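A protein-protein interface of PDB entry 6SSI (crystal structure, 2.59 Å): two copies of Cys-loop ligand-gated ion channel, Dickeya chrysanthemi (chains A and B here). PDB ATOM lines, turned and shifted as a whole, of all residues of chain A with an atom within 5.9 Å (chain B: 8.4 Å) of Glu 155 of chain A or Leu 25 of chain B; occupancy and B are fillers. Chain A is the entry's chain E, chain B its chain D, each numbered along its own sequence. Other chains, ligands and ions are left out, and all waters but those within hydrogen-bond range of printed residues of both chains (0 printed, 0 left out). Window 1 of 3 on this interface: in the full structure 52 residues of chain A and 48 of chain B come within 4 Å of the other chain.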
ATOM      1  N   TYR A  20     -23.015 -14.305  -6.349  1.00  0.00           N
ATOM      2  CA  TYR A  20     -22.844 -12.975  -5.760  1.00  0.00           C
ATOM      3  C   TYR A  20     -21.358 -12.522  -5.830  1.00  0.00           C
ATOM      4  O   TYR A  20     -20.530 -13.206  -6.423  1.00  0.00           O
ATOM      5  CB  TYR A  20     -23.345 -13.026  -4.296  1.00  0.00           C
ATOM      6  CG  TYR A  20     -22.438 -13.825  -3.381  1.00  0.00           C
ATOM      7  CD1 TYR A  20     -22.393 -15.218  -3.447  1.00  0.00           C
ATOM      8  CD2 TYR A  20     -21.619 -13.188  -2.455  1.00  0.00           C
ATOM      9  CE1 TYR A  20     -21.527 -15.952  -2.641  1.00  0.00           C
ATOM     10  CE2 TYR A  20     -20.764 -13.910  -1.631  1.00  0.00           C
ATOM     11  CZ  TYR A  20     -20.716 -15.292  -1.729  1.00  0.00           C
ATOM     12  OH  TYR A  20     -19.841 -15.980  -0.923  1.00  0.00           O
ATOM     13  N   GLU A 151     -36.357 -12.048  -8.086  1.00  0.00           N
ATOM     14  CA  GLU A 151     -37.181 -11.104  -7.346  1.00  0.00           C
ATOM     15  C   GLU A 151     -36.620  -9.714  -7.583  1.00  0.00           C
ATOM     16  O   GLU A 151     -35.472  -9.558  -8.022  1.00  0.00           O
ATOM     17  CB  GLU A 151     -37.231 -11.429  -5.836  1.00  0.00           C
ATOM     18  CG  GLU A 151     -38.019 -12.680  -5.469  1.00  0.00           C
ATOM     19  CD  GLU A 151     -37.309 -13.646  -4.536  1.00  0.00           C
ATOM     20  OE1 GLU A 151     -36.069 -13.539  -4.390  1.00  0.00           O
ATOM     21  OE2 GLU A 151     -37.992 -14.523  -3.959  1.00  0.00           O
ATOM     22  N   GLU A 152     -37.444  -8.704  -7.291  1.00  0.00           N
ATOM     23  CA  GLU A 152     -37.095  -7.291  -7.403  1.00  0.00           C
ATOM     24  C   GLU A 152     -36.024  -6.914  -6.387  1.00  0.00           C
ATOM     25  O   GLU A 152     -35.329  -5.919  -6.584  1.00  0.00           O
ATOM     26  CB  GLU A 152     -38.327  -6.421  -7.182  1.00  0.00           C
ATOM     27  CG  GLU A 152     -39.374  -6.526  -8.275  1.00  0.00           C
ATOM     28  CD  GLU A 152     -40.673  -5.809  -7.959  1.00  0.00           C
ATOM     29  OE1 GLU A 152     -40.662  -4.870  -7.129  1.00  0.00           O
ATOM     30  OE2 GLU A 152     -41.708  -6.188  -8.552  1.00  0.00           O
ATOM     31  N   ILE A 153     -35.886  -7.709  -5.307  1.00  0.00           N
ATOM     32  CA  ILE A 153     -34.895  -7.499  -4.246  1.00  0.00           C
ATOM     33  C   ILE A 153     -33.506  -8.078  -4.599  1.00  0.00           C
ATOM     34  O   ILE A 153     -32.575  -7.998  -3.790  1.00  0.00           O
ATOM     35  CB  ILE A 153     -35.412  -8.010  -2.875  1.00  0.00           C
ATOM     36  CG1 ILE A 153     -35.657  -9.541  -2.876  1.00  0.00           C
ATOM     37  CG2 ILE A 153     -36.646  -7.224  -2.437  1.00  0.00           C
ATOM     38  CD1 ILE A 153     -35.139 -10.246  -1.684  1.00  0.00           C
ATOM     39  N   ASP A 154     -33.385  -8.679  -5.791  1.00  0.00           N
ATOM     40  CA  ASP A 154     -32.143  -9.282  -6.255  1.00  0.00           C
ATOM     41  C   ASP A 154     -31.391  -8.340  -7.178  1.00  0.00           C
ATOM     42  O   ASP A 154     -31.985  -7.725  -8.068  1.00  0.00           O
ATOM     43  CB  ASP A 154     -32.412 -10.643  -6.919  1.00  0.00           C
ATOM     44  CG  ASP A 154     -32.804 -11.730  -5.938  1.00  0.00           C
ATOM     45  OD1 ASP A 154     -32.268 -11.731  -4.806  1.00  0.00           O
ATOM     46  OD2 ASP A 154     -33.629 -12.595  -6.309  1.00  0.00           O
ATOM     47  N   GLU A 155     -30.081  -8.208  -6.938  1.00  0.00           N
ATOM     48  CA  GLU A 155     -29.201  -7.366  -7.740  1.00  0.00           C
ATOM     49  C   GLU A 155     -29.149  -7.844  -9.203  1.00  0.00           C
ATOM     50  O   GLU A 155     -29.102  -7.023 -10.119  1.00  0.00           O
ATOM     51  CB  GLU A 155     -27.803  -7.341  -7.115  1.00  0.00           C
ATOM     52  CG  GLU A 155     -26.844  -6.384  -7.798  1.00  0.00           C
ATOM     53  CD  GLU A 155     -25.501  -6.260  -7.117  1.00  0.00           C
ATOM     54  OE1 GLU A 155     -25.265  -7.005  -6.139  1.00  0.00           O
ATOM     55  OE2 GLU A 155     -24.680  -5.425  -7.562  1.00  0.00           O
ATOM     56  N   TRP A 156     -29.174  -9.167  -9.410  1.00  0.00           N
ATOM     57  CA  TRP A 156     -29.129  -9.773 -10.731  1.00  0.00           C
ATOM     58  C   TRP A 156     -30.337 -10.637 -10.953  1.00  0.00           C
ATOM     59  O   TRP A 156     -30.785 -11.330 -10.034  1.00  0.00           O
ATOM     60  CB  TRP A 156     -27.867 -10.634 -10.882  1.00  0.00           C
ATOM     61  CG  TRP A 156     -26.603  -9.847 -10.846  1.00  0.00           C
ATOM     62  CD1 TRP A 156     -25.830  -9.580  -9.754  1.00  0.00           C
ATOM     63  CD2 TRP A 156     -25.976  -9.195 -11.954  1.00  0.00           C
ATOM     64  NE1 TRP A 156     -24.752  -8.809 -10.117  1.00  0.00           N
ATOM     65  CE2 TRP A 156     -24.810  -8.566 -11.465  1.00  0.00           C
ATOM     66  CE3 TRP A 156     -26.262  -9.116 -13.329  1.00  0.00           C
ATOM     67  CZ2 TRP A 156     -23.938  -7.855 -12.299  1.00  0.00           C
ATOM     68  CZ3 TRP A 156     -25.408  -8.399 -14.151  1.00  0.00           C
ATOM     69  CH2 TRP A 156     -24.266  -7.771 -13.635  1.00  0.00           C
ATOM     70  N   TRP A 157     -30.849 -10.616 -12.185  1.00  0.00           N
ATOM     71  CA  TRP A 157     -31.981 -11.433 -12.595  1.00  0.00           C
ATOM     72  C   TRP A 157     -31.476 -12.529 -13.495  1.00  0.00           C
ATOM     73  O   TRP A 157     -31.000 -12.263 -14.597  1.00  0.00           O
ATOM     74  CB  TRP A 157     -33.061 -10.597 -13.286  1.00  0.00           C
ATOM     75  CG  TRP A 157     -33.641  -9.522 -12.418  1.00  0.00           C
ATOM     76  CD1 TRP A 157     -33.825  -9.564 -11.066  1.00  0.00           C
ATOM     77  CD2 TRP A 157     -34.168  -8.263 -12.857  1.00  0.00           C
ATOM     78  NE1 TRP A 157     -34.400  -8.396 -10.631  1.00  0.00           N
ATOM     79  CE2 TRP A 157     -34.632  -7.582 -11.710  1.00  0.00           C
ATOM     80  CE3 TRP A 157     -34.292  -7.641 -14.114  1.00  0.00           C
ATOM     81  CZ2 TRP A 157     -35.252  -6.329 -11.787  1.00  0.00           C
ATOM     82  CZ3 TRP A 157     -34.872  -6.383 -14.182  1.00  0.00           C
ATOM     83  CH2 TRP A 157     -35.330  -5.734 -13.028  1.00  0.00           C
ATOM     84  N   VAL A 194     -29.120 -10.532 -15.974  1.00  0.00           N
ATOM     85  CA  VAL A 194     -29.316  -9.138 -16.359  1.00  0.00           C
ATOM     86  C   VAL A 194     -29.299  -8.354 -15.055  1.00  0.00           C
ATOM     87  O   VAL A 194     -29.908  -8.787 -14.075  1.00  0.00           O
ATOM     88  CB  VAL A 194     -30.629  -8.936 -17.182  1.00  0.00           C
ATOM     89  CG1 VAL A 194     -30.910  -7.463 -17.464  1.00  0.00           C
ATOM     90  CG2 VAL A 194     -30.596  -9.732 -18.487  1.00  0.00           C
ATOM     91  N   ARG A 195     -28.564  -7.228 -15.035  1.00  0.00           N
ATOM     92  CA  ARG A 195     -28.486  -6.366 -13.866  1.00  0.00           C
ATOM     93  C   ARG A 195     -29.830  -5.690 -13.631  1.00  0.00           C
ATOM     94  O   ARG A 195     -30.519  -5.323 -14.589  1.00  0.00           O
ATOM     95  CB  ARG A 195     -27.396  -5.293 -14.050  1.00  0.00           C
ATOM     96  CG  ARG A 195     -27.119  -4.478 -12.777  1.00  0.00           C
ATOM     97  CD  ARG A 195     -26.125  -3.355 -13.000  1.00  0.00           C
ATOM     98  NE  ARG A 195     -24.838  -3.875 -13.473  1.00  0.00           N
ATOM     99  CZ  ARG A 195     -23.864  -4.300 -12.676  1.00  0.00           C
ATOM    100  NH1 ARG A 195     -23.989  -4.246 -11.362  1.00  0.00           N
ATOM    101  NH2 ARG A 195     -22.736  -4.768 -13.205  1.00  0.00           N
ATOM    102  N   ASN A 196     -30.192  -5.530 -12.354  1.00  0.00           N
ATOM    103  CA  ASN A 196     -31.377  -4.794 -11.953  1.00  0.00           C
ATOM    104  C   ASN A 196     -30.975  -3.286 -11.972  1.00  0.00           C
ATOM    105  O   ASN A 196     -30.174  -2.849 -11.132  1.00  0.00           O
ATOM    106  CB  ASN A 196     -31.874  -5.249 -10.583  1.00  0.00           C
ATOM    107  CG  ASN A 196     -33.076  -4.490 -10.098  1.00  0.00           C
ATOM    108  OD1 ASN A 196     -33.693  -3.685 -10.819  1.00  0.00           O
ATOM    109  ND2 ASN A 196     -33.439  -4.744  -8.859  1.00  0.00           N
ATOM    110  N   PRO A 197     -31.459  -2.501 -12.973  1.00  0.00           N
ATOM    111  CA  PRO A 197     -31.011  -1.099 -13.095  1.00  0.00           C
ATOM    112  C   PRO A 197     -31.800  -0.048 -12.326  1.00  0.00           C
ATOM    113  O   PRO A 197     -31.481   1.139 -12.447  1.00  0.00           O
ATOM    114  CB  PRO A 197     -31.142  -0.839 -14.595  1.00  0.00           C
ATOM    115  CG  PRO A 197     -32.329  -1.656 -15.003  1.00  0.00           C
ATOM    116  CD  PRO A 197     -32.363  -2.868 -14.087  1.00  0.00           C
ATOM    117  N   TYR A 200     -29.932   2.622 -10.090  1.00  0.00           N
ATOM    118  CA  TYR A 200     -29.101   3.518 -10.887  1.00  0.00           C
ATOM    119  C   TYR A 200     -29.887   4.490 -11.751  1.00  0.00           C
ATOM    120  O   TYR A 200     -29.410   5.597 -11.989  1.00  0.00           O
ATOM    121  CB  TYR A 200     -28.104   2.717 -11.719  1.00  0.00           C
ATOM    122  CG  TYR A 200     -27.337   1.699 -10.904  1.00  0.00           C
ATOM    123  CD1 TYR A 200     -26.299   2.092 -10.060  1.00  0.00           C
ATOM    124  CD2 TYR A 200     -27.684   0.350 -10.932  1.00  0.00           C
ATOM    125  CE1 TYR A 200     -25.616   1.165  -9.277  1.00  0.00           C
ATOM    126  CE2 TYR A 200     -27.001  -0.587 -10.163  1.00  0.00           C
ATOM    127  CZ  TYR A 200     -25.962  -0.176  -9.341  1.00  0.00           C
ATOM    128  OH  TYR A 200     -25.263  -1.099  -8.603  1.00  0.00           O
ATOM    129  N   VAL B  22     -23.836  -7.786   9.067  1.00  0.00           N
ATOM    130  CA  VAL B  22     -24.847  -7.877   8.013  1.00  0.00           C
ATOM    131  C   VAL B  22     -24.262  -7.268   6.747  1.00  0.00           C
ATOM    132  O   VAL B  22     -23.727  -6.153   6.776  1.00  0.00           O
ATOM    133  CB  VAL B  22     -26.205  -7.228   8.400  1.00  0.00           C
ATOM    134  CG1 VAL B  22     -27.140  -7.092   7.188  1.00  0.00           C
ATOM    135  CG2 VAL B  22     -26.882  -7.993   9.536  1.00  0.00           C
ATOM    136  N   ASN B  23     -24.311  -8.031   5.653  1.00  0.00           N
ATOM    137  CA  ASN B  23     -23.837  -7.561   4.367  1.00  0.00           C
ATOM    138  C   ASN B  23     -25.054  -7.439   3.473  1.00  0.00           C
ATOM    139  O   ASN B  23     -25.584  -8.439   2.996  1.00  0.00           O
ATOM    140  CB  ASN B  23     -22.794  -8.493   3.792  1.00  0.00           C
ATOM    141  CG  ASN B  23     -22.113  -7.949   2.575  1.00  0.00           C
ATOM    142  OD1 ASN B  23     -22.724  -7.363   1.677  1.00  0.00           O
ATOM    143  ND2 ASN B  23     -20.819  -8.148   2.528  1.00  0.00           N
ATOM    144  N   THR B  24     -25.518  -6.202   3.288  1.00  0.00           N
ATOM    145  CA  THR B  24     -26.718  -5.893   2.513  1.00  0.00           C
ATOM    146  C   THR B  24     -26.690  -6.391   1.067  1.00  0.00           C
ATOM    147  O   THR B  24     -27.668  -7.008   0.644  1.00  0.00           O
ATOM    148  CB  THR B  24     -27.026  -4.417   2.577  1.00  0.00           C
ATOM    149  OG1 THR B  24     -25.875  -3.685   2.169  1.00  0.00           O
ATOM    150  CG2 THR B  24     -27.504  -3.995   3.946  1.00  0.00           C
ATOM    151  N   LEU B  25     -25.604  -6.138   0.313  1.00  0.00           N
ATOM    152  CA  LEU B  25     -25.512  -6.588  -1.076  1.00  0.00           C
ATOM    153  C   LEU B  25     -25.508  -8.101  -1.192  1.00  0.00           C
ATOM    154  O   LEU B  25     -26.209  -8.646  -2.049  1.00  0.00           O
ATOM    155  CB  LEU B  25     -24.274  -6.028  -1.774  1.00  0.00           C
ATOM    156  CG  LEU B  25     -24.475  -4.798  -2.646  1.00  0.00           C
ATOM    157  CD1 LEU B  25     -23.216  -4.474  -3.376  1.00  0.00           C
ATOM    158  CD2 LEU B  25     -25.619  -4.976  -3.633  1.00  0.00           C
ATOM    159  N   GLU B  26     -24.747  -8.775  -0.315  1.00  0.00           N
ATOM    160  CA  GLU B  26     -24.625 -10.225  -0.313  1.00  0.00           C
ATOM    161  C   GLU B  26     -25.776 -10.939   0.371  1.00  0.00           C
ATOM    162  O   GLU B  26     -25.882 -12.152   0.228  1.00  0.00           O
ATOM    163  CB  GLU B  26     -23.306 -10.656   0.315  1.00  0.00           C
ATOM    164  CG  GLU B  26     -22.077 -10.143  -0.408  1.00  0.00           C
ATOM    165  CD  GLU B  26     -20.755 -10.610   0.170  1.00  0.00           C
ATOM    166  OE1 GLU B  26     -20.750 -11.209   1.273  1.00  0.00           O
ATOM    167  OE2 GLU B  26     -19.716 -10.369  -0.487  1.00  0.00           O
ATOM    168  N   GLN B  27     -26.640 -10.204   1.103  1.00  0.00           N
ATOM    169  CA  GLN B  27     -27.765 -10.749   1.864  1.00  0.00           C
ATOM    170  C   GLN B  27     -27.261 -11.841   2.832  1.00  0.00           C
ATOM    171  O   GLN B  27     -27.747 -12.979   2.831  1.00  0.00           O
ATOM    172  CB  GLN B  27     -28.878 -11.247   0.938  1.00  0.00           C
ATOM    173  CG  GLN B  27     -29.563 -10.128   0.175  1.00  0.00           C
ATOM    174  CD  GLN B  27     -30.607 -10.672  -0.744  1.00  0.00           C
ATOM    175  OE1 GLN B  27     -31.633 -11.178  -0.317  1.00  0.00           O
ATOM    176  NE2 GLN B  27     -30.373 -10.575  -2.029  1.00  0.00           N
ATOM    177  N   THR B  28     -26.223 -11.490   3.612  1.00  0.00           N
ATOM    178  CA  THR B  28     -25.595 -12.406   4.560  1.00  0.00           C
ATOM    179  C   THR B  28     -25.447 -11.754   5.923  1.00  0.00           C
ATOM    180  O   THR B  28     -25.593 -10.534   6.073  1.00  0.00           O
ATOM    181  CB  THR B  28     -24.219 -12.915   4.055  1.00  0.00           C
ATOM    182  OG1 THR B  28     -23.314 -11.812   3.971  1.00  0.00           O
ATOM    183  CG2 THR B  28     -24.299 -13.686   2.730  1.00  0.00           C
ATOM    184  N   ASN B 108     -29.818 -15.562   3.605  1.00  0.00           N
ATOM    185  CA  ASN B 108     -31.267 -15.536   3.630  1.00  0.00           C
ATOM    186  C   ASN B 108     -31.748 -14.410   2.749  1.00  0.00           C
ATOM    187  O   ASN B 108     -31.025 -13.427   2.588  1.00  0.00           O
ATOM    188  CB  ASN B 108     -31.790 -15.346   5.046  1.00  0.00           C
ATOM    189  CG  ASN B 108     -33.272 -15.540   5.149  1.00  0.00           C
ATOM    190  OD1 ASN B 108     -33.911 -16.288   4.380  1.00  0.00           O
ATOM    191  ND2 ASN B 108     -33.845 -14.843   6.089  1.00  0.00           N
ATOM    192  N   MET B 110     -33.248 -11.205   2.063  1.00  0.00           N
ATOM    193  CA  MET B 110     -33.387 -10.003   2.883  1.00  0.00           C
ATOM    194  C   MET B 110     -33.823  -8.816   2.052  1.00  0.00           C
ATOM    195  O   MET B 110     -33.216  -8.507   1.024  1.00  0.00           O
ATOM    196  CB  MET B 110     -32.079  -9.679   3.633  1.00  0.00           C
ATOM    197  CG  MET B 110     -31.541 -10.830   4.457  1.00  0.00           C
ATOM    198  SD  MET B 110     -30.417 -10.436   5.819  1.00  0.00           S
ATOM    199  CE  MET B 110     -29.068  -9.851   5.006  1.00  0.00           C
ATOM    200  N   PHE B 112     -34.465  -4.819   2.159  1.00  0.00           N
ATOM    201  CA  PHE B 112     -34.118  -3.581   2.854  1.00  0.00           C
ATOM    202  C   PHE B 112     -34.812  -2.359   2.255  1.00  0.00           C
ATOM    203  O   PHE B 112     -34.327  -1.243   2.443  1.00  0.00           O
ATOM    204  CB  PHE B 112     -32.598  -3.373   2.817  1.00  0.00           C
ATOM    205  CG  PHE B 112     -31.783  -4.505   3.379  1.00  0.00           C
ATOM    206  CD1 PHE B 112     -31.524  -4.583   4.741  1.00  0.00           C
ATOM    207  CD2 PHE B 112     -31.252  -5.481   2.544  1.00  0.00           C
ATOM    208  CE1 PHE B 112     -30.766  -5.627   5.261  1.00  0.00           C
ATOM    209  CE2 PHE B 112     -30.485  -6.518   3.064  1.00  0.00           C
ATOM    210  CZ  PHE B 112     -30.246  -6.582   4.420  1.00  0.00           C
ATOM    211  N   PRO B 250     -25.865   1.614   3.615  1.00  0.00           N
ATOM    212  CA  PRO B 250     -25.441   0.388   2.933  1.00  0.00           C
ATOM    213  C   PRO B 250     -25.747   0.375   1.445  1.00  0.00           C
ATOM    214  O   PRO B 250     -26.682   1.038   0.995  1.00  0.00           O
ATOM    215  CB  PRO B 250     -26.220  -0.707   3.662  1.00  0.00           C
ATOM    216  CG  PRO B 250     -27.427  -0.041   4.174  1.00  0.00           C
ATOM    217  CD  PRO B 250     -26.969   1.338   4.562  1.00  0.00           C
ATOM    218  N   ARG B 251     -24.955  -0.410   0.692  1.00  0.00           N
ATOM    219  CA  ARG B 251     -25.117  -0.598  -0.745  1.00  0.00           C
ATOM    220  C   ARG B 251     -26.279  -1.521  -0.995  1.00  0.00           C
ATOM    221  O   ARG B 251     -26.346  -2.613  -0.424  1.00  0.00           O
ATOM    222  CB  ARG B 251     -23.842  -1.154  -1.397  1.00  0.00           C
ATOM    223  CG  ARG B 251     -22.607  -0.258  -1.267  1.00  0.00           C
ATOM    224  CD  ARG B 251     -22.552   0.929  -2.241  1.00  0.00           C
ATOM    225  NE  ARG B 251     -23.653   1.886  -2.062  1.00  0.00           N
ATOM    226  CZ  ARG B 251     -23.745   2.768  -1.068  1.00  0.00           C
ATOM    227  NH1 ARG B 251     -22.793   2.833  -0.142  1.00  0.00           N
ATOM    228  NH2 ARG B 251     -24.790   3.579  -0.984  1.00  0.00           N
ATOM    229  N   LEU B 252     -27.227  -1.059  -1.805  1.00  0.00           N
ATOM    230  CA  LEU B 252     -28.425  -1.821  -2.137  1.00  0.00           C
ATOM    231  C   LEU B 252     -28.746  -1.775  -3.631  1.00  0.00           C
ATOM    232  O   LEU B 252     -28.427  -0.775  -4.279  1.00  0.00           O
ATOM    233  CB  LEU B 252     -29.631  -1.312  -1.326  1.00  0.00           C
ATOM    234  CG  LEU B 252     -29.597  -1.580   0.168  1.00  0.00           C
ATOM    235  CD1 LEU B 252     -30.681  -0.845   0.851  1.00  0.00           C
ATOM    236  CD2 LEU B 252     -29.705  -3.060   0.471  1.00  0.00           C
ATOM    237  N   PRO B 253     -29.429  -2.808  -4.191  1.00  0.00           N
ATOM    238  CA  PRO B 253     -29.781  -2.765  -5.623  1.00  0.00           C
ATOM    239  C   PRO B 253     -31.090  -2.007  -5.901  1.00  0.00           C
ATOM    240  O   PRO B 253     -31.622  -2.064  -7.011  1.00  0.00           O
ATOM    241  CB  PRO B 253     -29.890  -4.247  -5.989  1.00  0.00           C
ATOM    242  CG  PRO B 253     -30.368  -4.904  -4.742  1.00  0.00           C
ATOM    243  CD  PRO B 253     -29.900  -4.066  -3.568  1.00  0.00           C
ATOM    244  N   TYR B 254     -31.617  -1.314  -4.881  1.00  0.00           N
ATOM    245  CA  TYR B 254     -32.856  -0.550  -4.959  1.00  0.00           C
ATOM    246  C   TYR B 254     -32.817   0.652  -4.042  1.00  0.00           C
ATOM    247  O   TYR B 254     -31.919   0.783  -3.207  1.00  0.00           O
ATOM    248  CB  TYR B 254     -34.090  -1.418  -4.637  1.00  0.00           C
ATOM    249  CG  TYR B 254     -33.890  -2.364  -3.475  1.00  0.00           C
ATOM    250  CD1 TYR B 254     -33.903  -1.903  -2.160  1.00  0.00           C
ATOM    251  CD2 TYR B 254     -33.657  -3.715  -3.690  1.00  0.00           C
ATOM    252  CE1 TYR B 254     -33.671  -2.769  -1.090  1.00  0.00           C
ATOM    253  CE2 TYR B 254     -33.425  -4.586  -2.631  1.00  0.00           C
ATOM    254  CZ  TYR B 254     -33.421  -4.111  -1.334  1.00  0.00           C
ATOM    255  OH  TYR B 254     -33.192  -5.011  -0.321  1.00  0.00           O
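The backbone NH (N) of Glu 26 of chain B sits at hydrogen-bond distance from the side-chain amide oxygen (OD1) of Asn 23 of chain B, 3.2 Å away. N of Asn 108 of chain B is in hydrogen-bond range of O of Gln 27 of chain B. OH of Tyr 254 of chain B is in hydrogen-bond range of N of Phe 112 of chain B, at 2.8 Å. The backbone carbonyl oxygen (O) of Glu 152 of chain A is in hydrogen-bond range of the side-chain amide nitrogen (ND2) of Asn 196 of chain A. The side-chain amide nitrogen of Asn 196 of chain A is in hydrogen-bond range of the backbone carbonyl oxygen of Asp 154 of chain A (3.4 Å). O of Glu 155 of chain A sits at hydrogen-bond distance from N of Asn 196 of chain A, 2.9 Å away.
Among the printed residues, merely in contact across the chains: Glu 155 of chain A with Leu 25 of chain B, Asp 154 of chain A with Gln 27 of chain B, Ile 153 of chain A with Tyr 254 of chain B, Glu 155 of chain A with Pro 253 of chain B, Tyr 20 of chain A with Glu 26 of chain B, Asn 196 of chain A with Pro 253 of chain B, Ile 153 of chain A with Met 110 of chain B, Ile 153 of chain A with Gln 27 of chain B and Ile 153 of chain A with Pro 253 of chain B.
Of the printed residues of chain B, Glu 155 of chain A touches Leu 25 and Pro 253. Of the printed residues of chain B, Tyr 20 of chain A touches Glu 26 (3.7 Å). Of the printed residues of chain A, Met 110 of chain B touches Ile 153. Glu 151 of chain A touches none of the printed residues of chain B.
Printed residues of chain A that touch a printed residue of chain B: Tyr 20, Ile 153, Asp 154, Glu 155 and Asn 196. Of the 15 printed residues of chain B, 6 touch a printed residue of chain A. Hydrophobic or aromatic side chains of chain B that line the printed part of chain A: Leu 25, Pro 253 and Tyr 254. Among the printed residues, no Asp or Glu carboxylate lies within 4 Å of a Lys or Arg side-chain nitrogen of the other chain.
No position is printed for both chains. Of the 9 pairs that touch across the chains among the printed residues, none has its exchanged pair printed and touching as well.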
